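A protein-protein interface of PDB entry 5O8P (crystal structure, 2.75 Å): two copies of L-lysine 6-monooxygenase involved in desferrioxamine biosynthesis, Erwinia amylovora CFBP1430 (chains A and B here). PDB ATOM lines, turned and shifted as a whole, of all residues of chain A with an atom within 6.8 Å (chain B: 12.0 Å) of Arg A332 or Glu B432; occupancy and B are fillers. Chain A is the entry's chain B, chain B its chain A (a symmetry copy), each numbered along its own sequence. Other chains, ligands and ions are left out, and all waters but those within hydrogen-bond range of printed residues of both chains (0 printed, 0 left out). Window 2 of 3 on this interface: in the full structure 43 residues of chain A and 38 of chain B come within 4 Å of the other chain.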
ATOM      1  N   SER A 194      17.871   7.861 -30.308  1.00  0.00           N
ATOM      2  CA  SER A 194      18.533   8.988 -29.647  1.00  0.00           C
ATOM      3  C   SER A 194      20.044   8.914 -29.839  1.00  0.00           C
ATOM      4  O   SER A 194      20.619   7.827 -29.823  1.00  0.00           O
ATOM      5  CB  SER A 194      18.197   9.012 -28.152  1.00  0.00           C
ATOM      6  OG  SER A 194      18.506   7.774 -27.538  1.00  0.00           O
ATOM      7  N   ILE A 195      20.667  10.075 -30.040  1.00  0.00           N
ATOM      8  CA  ILE A 195      22.121  10.194 -30.173  1.00  0.00           C
ATOM      9  C   ILE A 195      22.575  11.268 -29.204  1.00  0.00           C
ATOM     10  O   ILE A 195      21.887  12.274 -29.046  1.00  0.00           O
ATOM     11  CB  ILE A 195      22.538  10.622 -31.599  1.00  0.00           C
ATOM     12  CG1 ILE A 195      21.975   9.650 -32.646  1.00  0.00           C
ATOM     13  CG2 ILE A 195      24.059  10.750 -31.713  1.00  0.00           C
ATOM     14  CD1 ILE A 195      22.123  10.140 -34.072  1.00  0.00           C
ATOM     15  N   THR A 196      23.726  11.068 -28.573  1.00  0.00           N
ATOM     16  CA  THR A 196      24.285  12.061 -27.661  1.00  0.00           C
ATOM     17  C   THR A 196      25.748  12.314 -27.980  1.00  0.00           C
ATOM     18  O   THR A 196      26.580  11.431 -27.859  1.00  0.00           O
ATOM     19  CB  THR A 196      24.150  11.614 -26.196  1.00  0.00           C
ATOM     20  OG1 THR A 196      22.760  11.494 -25.866  1.00  0.00           O
ATOM     21  CG2 THR A 196      24.821  12.617 -25.239  1.00  0.00           C
ATOM     22  N   GLN A 221      16.367  11.840 -31.319  1.00  0.00           N
ATOM     23  CA  GLN A 221      16.690  12.852 -30.333  1.00  0.00           C
ATOM     24  C   GLN A 221      18.182  13.121 -30.481  1.00  0.00           C
ATOM     25  O   GLN A 221      18.971  12.184 -30.682  1.00  0.00           O
ATOM     26  CB  GLN A 221      16.374  12.359 -28.917  1.00  0.00           C
ATOM     27  CG  GLN A 221      16.770  13.335 -27.820  1.00  0.00           C
ATOM     28  CD  GLN A 221      16.280  12.902 -26.455  1.00  0.00           C
ATOM     29  OE1 GLN A 221      16.938  12.135 -25.762  1.00  0.00           O
ATOM     30  NE2 GLN A 221      15.129  13.412 -26.055  1.00  0.00           N
ATOM     31  N   ASN A 223      21.251  15.008 -28.566  1.00  0.00           N
ATOM     32  CA  ASN A 223      21.723  15.639 -27.342  1.00  0.00           C
ATOM     33  C   ASN A 223      23.183  16.035 -27.451  1.00  0.00           C
ATOM     34  O   ASN A 223      23.913  15.516 -28.294  1.00  0.00           O
ATOM     35  CB  ASN A 223      21.500  14.693 -26.174  1.00  0.00           C
ATOM     36  CG  ASN A 223      20.046  14.277 -26.050  1.00  0.00           C
ATOM     37  OD1 ASN A 223      19.146  15.086 -26.257  1.00  0.00           O
ATOM     38  ND2 ASN A 223      19.813  13.024 -25.733  1.00  0.00           N
ATOM     39  N   ASN A 298      18.549  18.299 -26.410  1.00  0.00           N
ATOM     40  CA  ASN A 298      18.953  18.723 -25.079  1.00  0.00           C
ATOM     41  C   ASN A 298      20.417  19.093 -25.147  1.00  0.00           C
ATOM     42  O   ASN A 298      21.182  18.453 -25.861  1.00  0.00           O
ATOM     43  CB  ASN A 298      18.735  17.600 -24.074  1.00  0.00           C
ATOM     44  CG  ASN A 298      17.303  17.136 -24.041  1.00  0.00           C
ATOM     45  OD1 ASN A 298      16.426  17.814 -23.502  1.00  0.00           O
ATOM     46  ND2 ASN A 298      17.046  15.999 -24.663  1.00  0.00           N
ATOM     47  N   ARG A 309      26.815   3.065 -17.997  1.00  0.00           N
ATOM     48  CA  ARG A 309      26.390   1.686 -17.965  1.00  0.00           C
ATOM     49  C   ARG A 309      25.377   1.421 -19.051  1.00  0.00           C
ATOM     50  O   ARG A 309      24.652   2.327 -19.477  1.00  0.00           O
ATOM     51  CB  ARG A 309      25.832   1.306 -16.593  1.00  0.00           C
ATOM     52  CG  ARG A 309      24.743   2.208 -16.043  1.00  0.00           C
ATOM     53  CD  ARG A 309      24.685   2.136 -14.511  1.00  0.00           C
ATOM     54  NE  ARG A 309      23.951   0.950 -14.064  1.00  0.00           N
ATOM     55  CZ  ARG A 309      22.619   0.825 -14.069  1.00  0.00           C
ATOM     56  NH1 ARG A 309      21.833   1.806 -14.514  1.00  0.00           N
ATOM     57  NH2 ARG A 309      22.054  -0.305 -13.647  1.00  0.00           N
ATOM     58  N   LEU A 311      22.174  -0.758 -20.359  1.00  0.00           N
ATOM     59  CA  LEU A 311      21.001  -1.429 -19.808  1.00  0.00           C
ATOM     60  C   LEU A 311      20.482  -2.483 -20.779  1.00  0.00           C
ATOM     61  O   LEU A 311      20.649  -2.342 -21.994  1.00  0.00           O
ATOM     62  CB  LEU A 311      19.904  -0.403 -19.519  1.00  0.00           C
ATOM     63  CG  LEU A 311      20.334   0.827 -18.706  1.00  0.00           C
ATOM     64  CD1 LEU A 311      19.215   1.849 -18.655  1.00  0.00           C
ATOM     65  CD2 LEU A 311      20.775   0.452 -17.300  1.00  0.00           C
ATOM     66  N   GLU A 313      17.433  -2.993 -21.593  1.00  0.00           N
ATOM     67  CA  GLU A 313      16.532  -2.199 -22.457  1.00  0.00           C
ATOM     68  C   GLU A 313      17.085  -1.873 -23.861  1.00  0.00           C
ATOM     69  O   GLU A 313      16.328  -1.870 -24.831  1.00  0.00           O
ATOM     70  CB  GLU A 313      16.188  -0.863 -21.781  1.00  0.00           C
ATOM     71  CG  GLU A 313      15.335  -0.943 -20.514  1.00  0.00           C
ATOM     72  CD  GLU A 313      15.112   0.425 -19.865  1.00  0.00           C
ATOM     73  OE1 GLU A 313      15.272   1.462 -20.562  1.00  0.00           O
ATOM     74  OE2 GLU A 313      14.770   0.455 -18.659  1.00  0.00           O
ATOM     75  N   GLU A 315      19.956   0.776 -24.105  1.00  0.00           N
ATOM     76  CA  GLU A 315      20.266   2.195 -23.894  1.00  0.00           C
ATOM     77  C   GLU A 315      21.441   2.355 -22.941  1.00  0.00           C
ATOM     78  O   GLU A 315      21.612   1.539 -22.034  1.00  0.00           O
ATOM     79  CB  GLU A 315      19.084   2.902 -23.228  1.00  0.00           C
ATOM     80  CG  GLU A 315      17.863   3.153 -24.087  1.00  0.00           C
ATOM     81  CD  GLU A 315      16.959   4.188 -23.441  1.00  0.00           C
ATOM     82  OE1 GLU A 315      16.410   3.911 -22.348  1.00  0.00           O
ATOM     83  OE2 GLU A 315      16.829   5.297 -24.004  1.00  0.00           O
ATOM     84  N   PHE A 316      22.217   3.420 -23.124  1.00  0.00           N
ATOM     85  CA  PHE A 316      23.165   3.861 -22.096  1.00  0.00           C
ATOM     86  C   PHE A 316      22.433   4.636 -21.001  1.00  0.00           C
ATOM     87  O   PHE A 316      21.407   5.280 -21.258  1.00  0.00           O
ATOM     88  CB  PHE A 316      24.224   4.794 -22.669  1.00  0.00           C
ATOM     89  CG  PHE A 316      25.295   4.110 -23.449  1.00  0.00           C
ATOM     90  CD1 PHE A 316      26.293   3.405 -22.795  1.00  0.00           C
ATOM     91  CD2 PHE A 316      25.347   4.226 -24.841  1.00  0.00           C
ATOM     92  CE1 PHE A 316      27.303   2.790 -23.525  1.00  0.00           C
ATOM     93  CE2 PHE A 316      26.358   3.617 -25.571  1.00  0.00           C
ATOM     94  CZ  PHE A 316      27.334   2.895 -24.912  1.00  0.00           C
ATOM     95  N   GLU A 317      22.974   4.581 -19.788  1.00  0.00           N
ATOM     96  CA  GLU A 317      22.619   5.524 -18.734  1.00  0.00           C
ATOM     97  C   GLU A 317      23.887   6.266 -18.328  1.00  0.00           C
ATOM     98  O   GLU A 317      24.748   5.713 -17.642  1.00  0.00           O
ATOM     99  CB  GLU A 317      21.994   4.823 -17.527  1.00  0.00           C
ATOM    100  CG  GLU A 317      21.316   5.790 -16.553  1.00  0.00           C
ATOM    101  CD  GLU A 317      21.510   5.452 -15.081  1.00  0.00           C
ATOM    102  OE1 GLU A 317      22.616   5.015 -14.693  1.00  0.00           O
ATOM    103  OE2 GLU A 317      20.550   5.641 -14.293  1.00  0.00           O
ATOM    104  N   LEU A 318      23.989   7.515 -18.774  1.00  0.00           N
ATOM    105  CA  LEU A 318      25.092   8.397 -18.409  1.00  0.00           C
ATOM    106  C   LEU A 318      24.809   9.020 -17.054  1.00  0.00           C
ATOM    107  O   LEU A 318      23.816   9.718 -16.909  1.00  0.00           O
ATOM    108  CB  LEU A 318      25.234   9.517 -19.438  1.00  0.00           C
ATOM    109  CG  LEU A 318      25.860   9.243 -20.814  1.00  0.00           C
ATOM    110  CD1 LEU A 318      25.853   7.783 -21.236  1.00  0.00           C
ATOM    111  CD2 LEU A 318      25.188  10.095 -21.880  1.00  0.00           C
ATOM    112  N   TYR A 329      23.123  14.019 -11.796  1.00  0.00           N
ATOM    113  CA  TYR A 329      21.932  13.676 -12.576  1.00  0.00           C
ATOM    114  C   TYR A 329      22.248  12.629 -13.637  1.00  0.00           C
ATOM    115  O   TYR A 329      23.403  12.480 -14.033  1.00  0.00           O
ATOM    116  CB  TYR A 329      21.322  14.921 -13.232  1.00  0.00           C
ATOM    117  CG  TYR A 329      22.100  15.546 -14.387  1.00  0.00           C
ATOM    118  CD1 TYR A 329      23.222  16.355 -14.160  1.00  0.00           C
ATOM    119  CD2 TYR A 329      21.679  15.370 -15.712  1.00  0.00           C
ATOM    120  CE1 TYR A 329      23.907  16.943 -15.223  1.00  0.00           C
ATOM    121  CE2 TYR A 329      22.362  15.958 -16.773  1.00  0.00           C
ATOM    122  CZ  TYR A 329      23.467  16.746 -16.521  1.00  0.00           C
ATOM    123  OH  TYR A 329      24.117  17.321 -17.576  1.00  0.00           O
ATOM    124  N   SER A 330      21.219  11.908 -14.085  1.00  0.00           N
ATOM    125  CA  SER A 330      21.368  10.861 -15.101  1.00  0.00           C
ATOM    126  C   SER A 330      20.645  11.243 -16.393  1.00  0.00           C
ATOM    127  O   SER A 330      19.695  12.032 -16.385  1.00  0.00           O
ATOM    128  CB  SER A 330      20.848   9.515 -14.586  1.00  0.00           C
ATOM    129  OG  SER A 330      19.442   9.559 -14.367  1.00  0.00           O
ATOM    130  N   ARG A 331      21.113  10.670 -17.498  1.00  0.00           N
ATOM    131  CA  ARG A 331      20.587  10.931 -18.830  1.00  0.00           C
ATOM    132  C   ARG A 331      20.656   9.624 -19.610  1.00  0.00           C
ATOM    133  O   ARG A 331      21.534   8.801 -19.342  1.00  0.00           O
ATOM    134  CB  ARG A 331      21.477  11.968 -19.501  1.00  0.00           C
ATOM    135  CG  ARG A 331      20.799  12.900 -20.454  1.00  0.00           C
ATOM    136  CD  ARG A 331      19.919  13.893 -19.715  1.00  0.00           C
ATOM    137  NE  ARG A 331      18.852  14.281 -20.623  1.00  0.00           N
ATOM    138  CZ  ARG A 331      17.703  14.829 -20.268  1.00  0.00           C
ATOM    139  NH1 ARG A 331      17.430  15.083 -18.991  1.00  0.00           N
ATOM    140  NH2 ARG A 331      16.805  15.078 -21.210  1.00  0.00           N
ATOM    141  N   ARG A 332      19.774   9.445 -20.585  1.00  0.00           N
ATOM    142  CA  ARG A 332      19.754   8.204 -21.364  1.00  0.00           C
ATOM    143  C   ARG A 332      19.976   8.464 -22.824  1.00  0.00           C
ATOM    144  O   ARG A 332      19.591   9.502 -23.326  1.00  0.00           O
ATOM    145  CB  ARG A 332      18.418   7.489 -21.199  1.00  0.00           C
ATOM    146  CG  ARG A 332      18.289   6.680 -19.926  1.00  0.00           C
ATOM    147  CD  ARG A 332      16.807   6.610 -19.587  1.00  0.00           C
ATOM    148  NE  ARG A 332      16.512   5.656 -18.541  1.00  0.00           N
ATOM    149  CZ  ARG A 332      16.509   4.330 -18.692  1.00  0.00           C
ATOM    150  NH1 ARG A 332      16.831   3.764 -19.857  1.00  0.00           N
ATOM    151  NH2 ARG A 332      16.195   3.544 -17.662  1.00  0.00           N
ATOM    152  N   THR A 333      20.585   7.504 -23.508  1.00  0.00           N
ATOM    153  CA  THR A 333      20.814   7.609 -24.950  1.00  0.00           C
ATOM    154  C   THR A 333      21.134   6.230 -25.553  1.00  0.00           C
ATOM    155  O   THR A 333      21.730   5.377 -24.883  1.00  0.00           O
ATOM    156  CB  THR A 333      21.930   8.638 -25.263  1.00  0.00           C
ATOM    157  OG1 THR A 333      21.916   8.982 -26.660  1.00  0.00           O
ATOM    158  CG2 THR A 333      23.313   8.123 -24.861  1.00  0.00           C
ATOM    159  N   GLU A 334      20.725   6.010 -26.802  1.00  0.00           N
ATOM    160  CA  GLU A 334      21.041   4.770 -27.500  1.00  0.00           C
ATOM    161  C   GLU A 334      22.410   4.919 -28.118  1.00  0.00           C
ATOM    162  O   GLU A 334      23.330   4.169 -27.786  1.00  0.00           O
ATOM    163  CB  GLU A 334      20.000   4.439 -28.568  1.00  0.00           C
ATOM    164  CG  GLU A 334      18.621   4.162 -27.992  1.00  0.00           C
ATOM    165  CD  GLU A 334      17.643   3.564 -29.000  1.00  0.00           C
ATOM    166  OE1 GLU A 334      17.957   3.534 -30.215  1.00  0.00           O
ATOM    167  OE2 GLU A 334      16.541   3.141 -28.570  1.00  0.00           O
ATOM    168  N   GLY A 335      22.532   5.905 -29.004  1.00  0.00           N
ATOM    169  CA  GLY A 335      23.798   6.242 -29.665  1.00  0.00           C
ATOM    170  C   GLY A 335      24.588   7.200 -28.809  1.00  0.00           C
ATOM    171  O   GLY A 335      24.019   8.060 -28.142  1.00  0.00           O
ATOM    172  N   THR B 426      19.604  23.586 -21.544  1.00  0.00           N
ATOM    173  CA  THR B 426      19.150  23.444 -20.178  1.00  0.00           C
ATOM    174  C   THR B 426      20.362  23.728 -19.296  1.00  0.00           C
ATOM    175  O   THR B 426      21.382  23.025 -19.383  1.00  0.00           O
ATOM    176  CB  THR B 426      18.641  22.032 -19.922  1.00  0.00           C
ATOM    177  OG1 THR B 426      17.704  21.693 -20.945  1.00  0.00           O
ATOM    178  CG2 THR B 426      17.972  21.924 -18.562  1.00  0.00           C
ATOM    179  N   PRO B 428      20.376  24.108 -15.536  1.00  0.00           N
ATOM    180  CA  PRO B 428      20.541  23.305 -14.328  1.00  0.00           C
ATOM    181  C   PRO B 428      20.657  21.812 -14.617  1.00  0.00           C
ATOM    182  O   PRO B 428      20.307  21.354 -15.706  1.00  0.00           O
ATOM    183  CB  PRO B 428      19.254  23.584 -13.552  1.00  0.00           C
ATOM    184  CG  PRO B 428      18.241  23.780 -14.620  1.00  0.00           C
ATOM    185  CD  PRO B 428      18.973  24.527 -15.709  1.00  0.00           C
ATOM    186  N   ALA B 429      21.136  21.068 -13.625  1.00  0.00           N
ATOM    187  CA  ALA B 429      21.067  19.617 -13.652  1.00  0.00           C
ATOM    188  C   ALA B 429      19.615  19.222 -13.838  1.00  0.00           C
ATOM    189  O   ALA B 429      18.720  19.919 -13.360  1.00  0.00           O
ATOM    190  CB  ALA B 429      21.609  19.026 -12.358  1.00  0.00           C
ATOM    191  N   GLN B 430      19.390  18.122 -14.551  1.00  0.00           N
ATOM    192  CA  GLN B 430      18.044  17.617 -14.805  1.00  0.00           C
ATOM    193  C   GLN B 430      18.069  16.149 -15.224  1.00  0.00           C
ATOM    194  O   GLN B 430      18.475  15.831 -16.337  1.00  0.00           O
ATOM    195  CB  GLN B 430      17.366  18.465 -15.887  1.00  0.00           C
ATOM    196  CG  GLN B 430      15.966  17.995 -16.263  1.00  0.00           C
ATOM    197  CD  GLN B 430      15.444  18.668 -17.503  1.00  0.00           C
ATOM    198  OE1 GLN B 430      15.426  19.891 -17.581  1.00  0.00           O
ATOM    199  NE2 GLN B 430      15.007  17.869 -18.482  1.00  0.00           N
ATOM    200  N   SER B 431      17.607  15.275 -14.336  1.00  0.00           N
ATOM    201  CA  SER B 431      17.553  13.840 -14.610  1.00  0.00           C
ATOM    202  C   SER B 431      16.450  13.460 -15.596  1.00  0.00           C
ATOM    203  O   SER B 431      15.548  14.242 -15.885  1.00  0.00           O
ATOM    204  CB  SER B 431      17.354  13.046 -13.310  1.00  0.00           C
ATOM    205  OG  SER B 431      18.525  13.067 -12.517  1.00  0.00           O
ATOM    206  N   GLU B 432      16.512  12.204 -16.043  1.00  0.00           N
ATOM    207  CA  GLU B 432      15.582  11.629 -17.004  1.00  0.00           C
ATOM    208  C   GLU B 432      15.212  10.195 -16.584  1.00  0.00           C
ATOM    209  O   GLU B 432      14.138   9.944 -16.039  1.00  0.00           O
ATOM    210  CB  GLU B 432      16.279  11.613 -18.362  1.00  0.00           C
ATOM    211  CG  GLU B 432      15.411  11.237 -19.553  1.00  0.00           C
ATOM    212  CD  GLU B 432      16.217  10.910 -20.806  1.00  0.00           C
ATOM    213  OE1 GLU B 432      17.457  11.090 -20.818  1.00  0.00           O
ATOM    214  OE2 GLU B 432      15.602  10.461 -21.794  1.00  0.00           O
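N of Arg A332 lies within hydrogen-bond range of OE1 of Glu B432, at 2.9 Å.
NE of Arg A331 lies within salt-bridge range of OE1 of Glu B432, at 3.5 Å.
O of Gln B430 is in hydrogen-bond range of NH1 of Arg A331, at 2.9 Å.
O of Ser A330 lies within hydrogen-bond range of N of Glu B432 (3.2 Å).
OG of Ser B431 is in hydrogen-bond range of N of Ser A330.
The side-chain carboxylate (OE1) of Glu A315 lies within salt-bridge range of the guanidinium group (NH1) of Arg A332, at 2.5 Å.
N of Leu A318 sits at hydrogen-bond distance from O of Arg A331 (2.8 Å).
The side-chain carboxylate of Glu A313 lies within salt-bridge range of the guanidinium group of Arg A332, 2.9 Å away.
Among the printed residues, pairs that only touch across the chains: Tyr A329 with Ala B429 (3.6 Å), Tyr A329 with Gln B430 (3.3 Å), Tyr A329 with Ser B431 (3.4 Å), Ser A330 with Gln B430 (3.99 Å) and Arg A331 with Ser B431 (3.7 Å).
No residue of chain B comes within 4 Å of Ser A194.
No residue of chain B comes within 4 Å of Glu A315.
Glu A317 touches none of the printed residues of chain B.
Of the printed residues of chain B, Tyr A329 touches Ala B429 (3.6 Å), Gln B430 (3.3 Å) and Ser B431 (3.4 Å).
Printed residues of chain B within 4 Å of Ser A330: Gln B430, Ser B431 and Glu B432.
Of the printed residues of chain B, Arg A331 touches Gln B430 (2.9 Å), Ser B431 (3.7 Å) and Glu B432 (3.5 Å).
Of chain B, only Glu B432 comes within 4 Å of Arg A332.
Of the printed residues of chain A, Ala B429 touches Tyr A329 (3.6 Å).
Printed residues of chain A within 4 Å of Gln B430: Tyr A329, Ser A330 and Arg A331.
Glu B432 touches three residues of chain A.
The nearest residue of chain B that does not touch Arg A332 is Ser B431 (7.2 Å).
The nearest residue of chain A that does not touch Glu B432 is Gln A221 (4.5 Å).
Hydrophobic or aromatic side chains of chain B within 4 Å of the printed part of chain A: Ala B429.
No position is printed for both chains.
Of the 10 pairs that touch across the chains among the printed residues, none has its exchanged pair printed and touching as well.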
